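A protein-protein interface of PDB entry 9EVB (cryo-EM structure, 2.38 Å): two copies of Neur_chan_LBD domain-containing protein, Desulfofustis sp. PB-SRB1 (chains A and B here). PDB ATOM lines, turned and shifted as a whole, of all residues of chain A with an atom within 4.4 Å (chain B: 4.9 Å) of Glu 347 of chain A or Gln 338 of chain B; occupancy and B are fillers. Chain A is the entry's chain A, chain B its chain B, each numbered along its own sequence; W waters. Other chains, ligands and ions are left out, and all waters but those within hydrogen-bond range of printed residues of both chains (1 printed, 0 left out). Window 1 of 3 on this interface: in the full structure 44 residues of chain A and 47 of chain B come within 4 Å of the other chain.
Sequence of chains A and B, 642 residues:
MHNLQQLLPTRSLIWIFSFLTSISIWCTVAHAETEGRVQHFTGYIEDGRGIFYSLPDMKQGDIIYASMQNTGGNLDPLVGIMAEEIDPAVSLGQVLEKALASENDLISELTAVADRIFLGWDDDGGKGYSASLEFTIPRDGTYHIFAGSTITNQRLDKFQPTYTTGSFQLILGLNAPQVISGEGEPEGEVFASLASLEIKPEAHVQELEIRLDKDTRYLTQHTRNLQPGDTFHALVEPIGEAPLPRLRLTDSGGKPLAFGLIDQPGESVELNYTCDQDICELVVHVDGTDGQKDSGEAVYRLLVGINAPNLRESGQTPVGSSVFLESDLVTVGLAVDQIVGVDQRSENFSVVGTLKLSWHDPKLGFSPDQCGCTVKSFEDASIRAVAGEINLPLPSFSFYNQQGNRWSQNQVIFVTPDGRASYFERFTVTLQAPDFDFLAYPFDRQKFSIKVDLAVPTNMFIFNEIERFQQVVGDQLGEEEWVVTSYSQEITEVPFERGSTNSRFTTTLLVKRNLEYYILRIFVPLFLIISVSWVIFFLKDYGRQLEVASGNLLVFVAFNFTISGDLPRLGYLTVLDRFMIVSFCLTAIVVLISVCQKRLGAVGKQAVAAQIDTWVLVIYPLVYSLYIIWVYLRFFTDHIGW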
ATOM      1  N   ASP A 343      14.878 -34.901  -9.866  1.00  0.00           N
ATOM      2  CA  ASP A 343      14.875 -33.555 -10.439  1.00  0.00           C
ATOM      3  C   ASP A 343      16.186 -32.889 -10.053  1.00  0.00           C
ATOM      4  O   ASP A 343      16.367 -32.491  -8.900  1.00  0.00           O
ATOM      5  CB  ASP A 343      13.685 -32.742  -9.927  1.00  0.00           C
ATOM      6  CG  ASP A 343      13.507 -31.408 -10.659  1.00  0.00           C
ATOM      7  OD1 ASP A 343      14.497 -30.834 -11.162  1.00  0.00           O
ATOM      8  OD2 ASP A 343      12.360 -30.924 -10.737  1.00  0.00           O
ATOM      9  N   GLN A 344      17.085 -32.749 -11.024  1.00  0.00           N
ATOM     10  CA  GLN A 344      18.431 -32.277 -10.733  1.00  0.00           C
ATOM     11  C   GLN A 344      18.501 -30.759 -10.612  1.00  0.00           C
ATOM     12  O   GLN A 344      19.454 -30.230 -10.031  1.00  0.00           O
ATOM     13  CB  GLN A 344      19.386 -32.782 -11.813  1.00  0.00           C
ATOM     14  CG  GLN A 344      19.536 -34.305 -11.846  1.00  0.00           C
ATOM     15  CD  GLN A 344      20.109 -34.818 -13.171  1.00  0.00           C
ATOM     16  OE1 GLN A 344      20.617 -34.050 -13.979  1.00  0.00           O
ATOM     17  NE2 GLN A 344      19.995 -36.108 -13.410  1.00  0.00           N
ATOM     18  N   ARG A 345      17.563 -30.047 -11.233  1.00  0.00           N
ATOM     19  CA  ARG A 345      17.514 -28.592 -11.130  1.00  0.00           C
ATOM     20  C   ARG A 345      16.921 -28.187  -9.786  1.00  0.00           C
ATOM     21  O   ARG A 345      17.547 -27.458  -9.009  1.00  0.00           O
ATOM     22  CB  ARG A 345      16.713 -27.991 -12.287  1.00  0.00           C
ATOM     23  CG  ARG A 345      16.966 -26.501 -12.531  1.00  0.00           C
ATOM     24  CD  ARG A 345      16.849 -26.143 -14.011  1.00  0.00           C
ATOM     25  NE  ARG A 345      16.458 -24.754 -14.228  1.00  0.00           N
ATOM     26  CZ  ARG A 345      17.281 -23.789 -14.616  1.00  0.00           C
ATOM     27  NH1 ARG A 345      18.571 -24.011 -14.799  1.00  0.00           N
ATOM     28  NH2 ARG A 345      16.795 -22.569 -14.829  1.00  0.00           N
ATOM     29  N   SER A 346      15.722 -28.689  -9.490  1.00  0.00           N
ATOM     30  CA  SER A 346      14.997 -28.388  -8.259  1.00  0.00           C
ATOM     31  C   SER A 346      15.599 -29.094  -7.051  1.00  0.00           C
ATOM     32  O   SER A 346      15.372 -28.669  -5.909  1.00  0.00           O
ATOM     33  CB  SER A 346      13.528 -28.778  -8.414  1.00  0.00           C
ATOM     34  OG  SER A 346      12.729 -28.187  -7.405  1.00  0.00           O
ATOM     35  N   GLU A 347      16.369 -30.154  -7.294  1.00  0.00           N
ATOM     36  CA  GLU A 347      17.040 -30.963  -6.277  1.00  0.00           C
ATOM     37  C   GLU A 347      16.046 -31.695  -5.353  1.00  0.00           C
ATOM     38  O   GLU A 347      15.957 -31.424  -4.156  1.00  0.00           O
ATOM     39  CB  GLU A 347      18.076 -30.114  -5.512  1.00  0.00           C
ATOM     40  CG  GLU A 347      19.276 -29.724  -6.406  1.00  0.00           C
ATOM     41  CD  GLU A 347      20.300 -28.810  -5.725  1.00  0.00           C
ATOM     42  OE1 GLU A 347      20.659 -29.044  -4.554  1.00  0.00           O
ATOM     43  OE2 GLU A 347      20.646 -27.768  -6.322  1.00  0.00           O
ATOM     44  N   ASN A 348      15.298 -32.650  -5.934  1.00  0.00           N
ATOM     45  CA  ASN A 348      14.432 -33.568  -5.179  1.00  0.00           C
ATOM     46  C   ASN A 348      14.394 -34.936  -5.870  1.00  0.00           C
ATOM     47  O   ASN A 348      14.781 -35.068  -7.031  1.00  0.00           O
ATOM     48  CB  ASN A 348      12.994 -33.022  -5.015  1.00  0.00           C
ATOM     49  CG  ASN A 348      12.288 -32.799  -6.352  1.00  0.00           C
ATOM     50  OD1 ASN A 348      12.049 -33.736  -7.103  1.00  0.00           O
ATOM     51  ND2 ASN A 348      11.911 -31.573  -6.620  1.00  0.00           N
ATOM     52  N   GLN A 432      12.571 -33.538  -0.707  1.00  0.00           N
ATOM     53  CA  GLN A 432      13.565 -32.510  -1.002  1.00  0.00           C
ATOM     54  C   GLN A 432      14.983 -32.995  -0.706  1.00  0.00           C
ATOM     55  O   GLN A 432      15.208 -33.714   0.269  1.00  0.00           O
ATOM     56  CB  GLN A 432      13.258 -31.230  -0.223  1.00  0.00           C
ATOM     57  CG  GLN A 432      12.179 -30.351  -0.886  1.00  0.00           C
ATOM     58  CD  GLN A 432      11.605 -29.265   0.042  1.00  0.00           C
ATOM     59  OE1 GLN A 432      11.965 -29.158   1.205  1.00  0.00           O
ATOM     60  NE2 GLN A 432      10.641 -28.521  -0.467  1.00  0.00           N
ATOM     61  N   ALA A 433      15.956 -32.572  -1.526  1.00  0.00           N
ATOM     62  CA  ALA A 433      17.330 -33.039  -1.331  1.00  0.00           C
ATOM     63  C   ALA A 433      18.390 -32.018  -1.735  1.00  0.00           C
ATOM     64  O   ALA A 433      19.083 -32.224  -2.732  1.00  0.00           O
ATOM     65  CB  ALA A 433      17.569 -34.318  -2.136  1.00  0.00           C
ATOM     66  N   PRO A 434      18.553 -30.917  -0.998  1.00  0.00           N
ATOM     67  CA  PRO A 434      19.547 -29.903  -1.400  1.00  0.00           C
ATOM     68  C   PRO A 434      20.987 -30.340  -1.228  1.00  0.00           C
ATOM     69  O   PRO A 434      21.883 -29.673  -1.755  1.00  0.00           O
ATOM     70  CB  PRO A 434      19.216 -28.717  -0.480  1.00  0.00           C
ATOM     71  CG  PRO A 434      18.551 -29.404   0.689  1.00  0.00           C
ATOM     72  CD  PRO A 434      17.657 -30.382   0.033  1.00  0.00           C
ATOM     73  N   PHE A 436      22.401 -32.536  -2.777  1.00  0.00           N
ATOM     74  CA  PHE A 436      22.856 -33.039  -4.075  1.00  0.00           C
ATOM     75  C   PHE A 436      24.028 -32.195  -4.561  1.00  0.00           C
ATOM     76  O   PHE A 436      24.060 -30.984  -4.324  1.00  0.00           O
ATOM     77  CB  PHE A 436      21.752 -32.944  -5.139  1.00  0.00           C
ATOM     78  CG  PHE A 436      20.708 -34.037  -5.112  1.00  0.00           C
ATOM     79  CD1 PHE A 436      20.893 -35.225  -4.428  1.00  0.00           C
ATOM     80  CD2 PHE A 436      19.544 -33.873  -5.862  1.00  0.00           C
ATOM     81  CE1 PHE A 436      19.925 -36.214  -4.461  1.00  0.00           C
ATOM     82  CE2 PHE A 436      18.577 -34.853  -5.904  1.00  0.00           C
ATOM     83  CZ  PHE A 436      18.766 -36.028  -5.201  1.00  0.00           C
ATOM     84  N   VAL B 336      15.326 -18.755   5.410  1.00  0.00           N
ATOM     85  CA  VAL B 336      15.212 -19.393   4.102  1.00  0.00           C
ATOM     86  C   VAL B 336      16.133 -20.602   4.018  1.00  0.00           C
ATOM     87  O   VAL B 336      17.328 -20.505   4.324  1.00  0.00           O
ATOM     88  CB  VAL B 336      15.496 -18.407   2.959  1.00  0.00           C
ATOM     89  CG1 VAL B 336      15.605 -19.157   1.652  1.00  0.00           C
ATOM     90  CG2 VAL B 336      14.371 -17.389   2.860  1.00  0.00           C
ATOM     91  N   ASP B 337      15.587 -21.737   3.593  1.00  0.00           N
ATOM     92  CA  ASP B 337      16.387 -22.937   3.383  1.00  0.00           C
ATOM     93  C   ASP B 337      16.892 -23.050   1.947  1.00  0.00           C
ATOM     94  O   ASP B 337      18.063 -23.379   1.732  1.00  0.00           O
ATOM     95  CB  ASP B 337      15.580 -24.187   3.746  1.00  0.00           C
ATOM     96  CG  ASP B 337      15.362 -24.346   5.250  1.00  0.00           C
ATOM     97  OD1 ASP B 337      16.324 -24.675   5.983  1.00  0.00           O
ATOM     98  OD2 ASP B 337      14.214 -24.151   5.701  1.00  0.00           O
ATOM     99  N   GLN B 338      16.031 -22.771   0.969  1.00  0.00           N
ATOM    100  CA  GLN B 338      16.317 -23.118  -0.415  1.00  0.00           C
ATOM    101  C   GLN B 338      15.444 -22.286  -1.339  1.00  0.00           C
ATOM    102  O   GLN B 338      14.226 -22.222  -1.149  1.00  0.00           O
ATOM    103  CB  GLN B 338      16.068 -24.616  -0.641  1.00  0.00           C
ATOM    104  CG  GLN B 338      16.490 -25.151  -2.000  1.00  0.00           C
ATOM    105  CD  GLN B 338      16.160 -26.631  -2.168  1.00  0.00           C
ATOM    106  OE1 GLN B 338      15.519 -27.224  -1.317  1.00  0.00           O
ATOM    107  NE2 GLN B 338      16.563 -27.212  -3.282  1.00  0.00           N
ATOM    108  N   ILE B 339      16.066 -21.647  -2.328  1.00  0.00           N
ATOM    109  CA  ILE B 339      15.340 -21.107  -3.474  1.00  0.00           C
ATOM    110  C   ILE B 339      15.153 -22.251  -4.464  1.00  0.00           C
ATOM    111  O   ILE B 339      16.130 -22.778  -4.998  1.00  0.00           O
ATOM    112  CB  ILE B 339      16.089 -19.941  -4.129  1.00  0.00           C
ATOM    113  CG1 ILE B 339      16.195 -18.757  -3.170  1.00  0.00           C
ATOM    114  CG2 ILE B 339      15.356 -19.529  -5.382  1.00  0.00           C
ATOM    115  CD1 ILE B 339      17.445 -17.908  -3.389  1.00  0.00           C
ATOM    116  N   VAL B 340      13.905 -22.655  -4.696  1.00  0.00           N
ATOM    117  CA  VAL B 340      13.646 -23.849  -5.498  1.00  0.00           C
ATOM    118  C   VAL B 340      13.212 -23.576  -6.938  1.00  0.00           C
ATOM    119  O   VAL B 340      13.055 -24.544  -7.696  1.00  0.00           O
ATOM    120  CB  VAL B 340      12.592 -24.750  -4.831  1.00  0.00           C
ATOM    121  CG1 VAL B 340      13.204 -25.550  -3.669  1.00  0.00           C
ATOM    122  CG2 VAL B 340      11.427 -23.882  -4.392  1.00  0.00           C
ATOM    123  N   SER B 350       9.833 -19.354  -6.202  1.00  0.00           N
ATOM    124  CA  SER B 350       9.387 -20.311  -5.187  1.00  0.00           C
ATOM    125  C   SER B 350      10.478 -20.548  -4.142  1.00  0.00           C
ATOM    126  O   SER B 350      11.663 -20.623  -4.484  1.00  0.00           O
ATOM    127  CB  SER B 350       9.006 -21.653  -5.830  1.00  0.00           C
ATOM    128  OG  SER B 350       7.975 -21.523  -6.796  1.00  0.00           O
ATOM    129  N   VAL B 351      10.080 -20.722  -2.872  1.00  0.00           N
ATOM    130  CA  VAL B 351      11.035 -20.785  -1.766  1.00  0.00           C
ATOM    131  C   VAL B 351      10.565 -21.714  -0.638  1.00  0.00           C
ATOM    132  O   VAL B 351       9.365 -21.875  -0.393  1.00  0.00           O
ATOM    133  CB  VAL B 351      11.313 -19.365  -1.227  1.00  0.00           C
ATOM    134  CG1 VAL B 351      10.025 -18.745  -0.681  1.00  0.00           C
ATOM    135  CG2 VAL B 351      12.460 -19.361  -0.204  1.00  0.00           C
ATOM    136  N   VAL B 352      11.542 -22.273   0.090  1.00  0.00           N
ATOM    137  CA  VAL B 352      11.344 -23.184   1.218  1.00  0.00           C
ATOM    138  C   VAL B 352      11.936 -22.533   2.466  1.00  0.00           C
ATOM    139  O   VAL B 352      13.056 -22.011   2.423  1.00  0.00           O
ATOM    140  CB  VAL B 352      12.002 -24.549   0.940  1.00  0.00           C
ATOM    141  CG1 VAL B 352      11.952 -25.468   2.162  1.00  0.00           C
ATOM    142  CG2 VAL B 352      11.361 -25.206  -0.274  1.00  0.00           C
ATOM    143  N   LEU B 477      25.104 -27.950   0.202  1.00  0.00           N
ATOM    144  CA  LEU B 477      26.181 -28.555  -0.585  1.00  0.00           C
ATOM    145  C   LEU B 477      25.955 -28.390  -2.084  1.00  0.00           C
ATOM    146  O   LEU B 477      24.826 -28.481  -2.579  1.00  0.00           O
ATOM    147  CB  LEU B 477      26.325 -30.054  -0.268  1.00  0.00           C
ATOM    148  CG  LEU B 477      26.602 -30.432   1.192  1.00  0.00           C
ATOM    149  CD1 LEU B 477      26.420 -31.936   1.574  1.00  0.00           C
ATOM    150  CD2 LEU B 477      27.954 -29.888   1.746  1.00  0.00           C
ATOM    151  N   GLU B 479      26.701 -26.367  -5.958  1.00  0.00           N
ATOM    152  CA  GLU B 479      26.490 -25.027  -6.486  1.00  0.00           C
ATOM    153  C   GLU B 479      25.006 -24.699  -6.632  1.00  0.00           C
ATOM    154  O   GLU B 479      24.141 -25.579  -6.677  1.00  0.00           O
ATOM    155  CB  GLU B 479      27.144 -24.847  -7.858  1.00  0.00           C
ATOM    156  CG  GLU B 479      28.623 -25.125  -7.957  1.00  0.00           C
ATOM    157  CD  GLU B 479      29.428 -24.521  -6.839  1.00  0.00           C
ATOM    158  OE1 GLU B 479      29.338 -23.294  -6.620  1.00  0.00           O
ATOM    159  OE2 GLU B 479      30.122 -25.296  -6.152  1.00  0.00           O
ATOM    160  N   GLU B 480      24.735 -23.402  -6.755  1.00  0.00           N
ATOM    161  CA  GLU B 480      23.407 -22.862  -6.993  1.00  0.00           C
ATOM    162  C   GLU B 480      23.453 -21.965  -8.226  1.00  0.00           C
ATOM    163  O   GLU B 480      24.495 -21.386  -8.555  1.00  0.00           O
ATOM    164  CB  GLU B 480      22.912 -22.086  -5.761  1.00  0.00           C
ATOM    165  CG  GLU B 480      22.284 -22.948  -4.683  1.00  0.00           C
ATOM    166  CD  GLU B 480      23.298 -23.724  -3.868  1.00  0.00           C
ATOM    167  OE1 GLU B 480      24.313 -23.158  -3.420  1.00  0.00           O
ATOM    168  OE2 GLU B 480      23.081 -24.942  -3.708  1.00  0.00           O
HETATM  169  O   HOH W   1      14.711 -27.849   1.150  1.00  0.00           O
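O of Gln 338 of chain B lies within hydrogen-bond range of N of Val 352 of chain B (3.0 Å).
OD1 of Asp 343 of chain A is in hydrogen-bond range of N of Ser 346 of chain A, at 3.0 Å.
The backbone carbonyl oxygen of Glu 347 of chain A sits at hydrogen-bond distance from the backbone NH of Ala 433 of chain A (2.9 Å).
N of Val 340 of chain B lies within hydrogen-bond range of O of Ser 350 of chain B.
The backbone NH (N) of Asp 337 of chain B sits at hydrogen-bond distance from the backbone carbonyl oxygen (O) of Val 352 of chain B.
No position is printed for both chains.
Of the 6 pairs that touch across the chains among the printed residues, none has its exchanged pair printed and touching as well.
Among the printed residues, merely in contact across the chains: Gln 432 of chain A with Val 352 of chain B (3.4 Å), Ser 346 of chain A with Val 340 of chain B (3.7 Å) and Glu 347 of chain A with Gln 338 of chain B (3.96 Å).
Of the printed residues of chain B, Glu 347 of chain A touches Gln 338 (3.96 Å).
Gln 338 of chain B touches just these residues of chain A: Ser 346 (3.2 Å) and Glu 347 (3.96 Å).
Of the printed residues of chain B, Gln 432 of chain A touches Val 352.
Of the printed residues of chain A, Leu 477 of chain B touches Pro 434 (3.3 Å) and Phe 436 (3.1 Å).
Of the printed residues of chain A, Val 340 of chain B touches Ser 346 (3.7 Å).
Of the printed residues of chain A, Val 352 of chain B touches Gln 432 (3.4 Å).
The nearest residue of chain B that does not touch Glu 347 of chain A is Glu 479 of chain B (4.1 Å).
The nearest residue of chain A that does not touch Gln 338 of chain B is Pro 434 of chain A (4.05 Å).
The nearest printed residue of chain B that does not touch Phe 436 of chain A is Glu 479 of chain B (5.6 Å).
Water W1 bridges OE1 of Gln 338 of chain B and OE1 of Gln 432 of chain A.
Printed residues of chain A that touch a printed residue of chain B: Ser 346, Glu 347, Gln 432, Pro 434 and Phe 436.
Among the printed residues, 6 pairs touch across the chains.
The backbone carbonyl oxygen of Leu 477 of chain B lies close to the backbone carbonyl oxygen of Pro 434 of chain A.
The backbone carbonyl oxygen (O) of Ser 346 of chain A is in hydrogen-bond range of the side-chain amide nitrogen (NE2) of Gln 338 of chain B (3.2 Å).
The backbone carbonyl oxygen of Phe 436 of chain A lies close to the backbone carbonyl oxygen of Leu 477 of chain B (3.1 Å).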
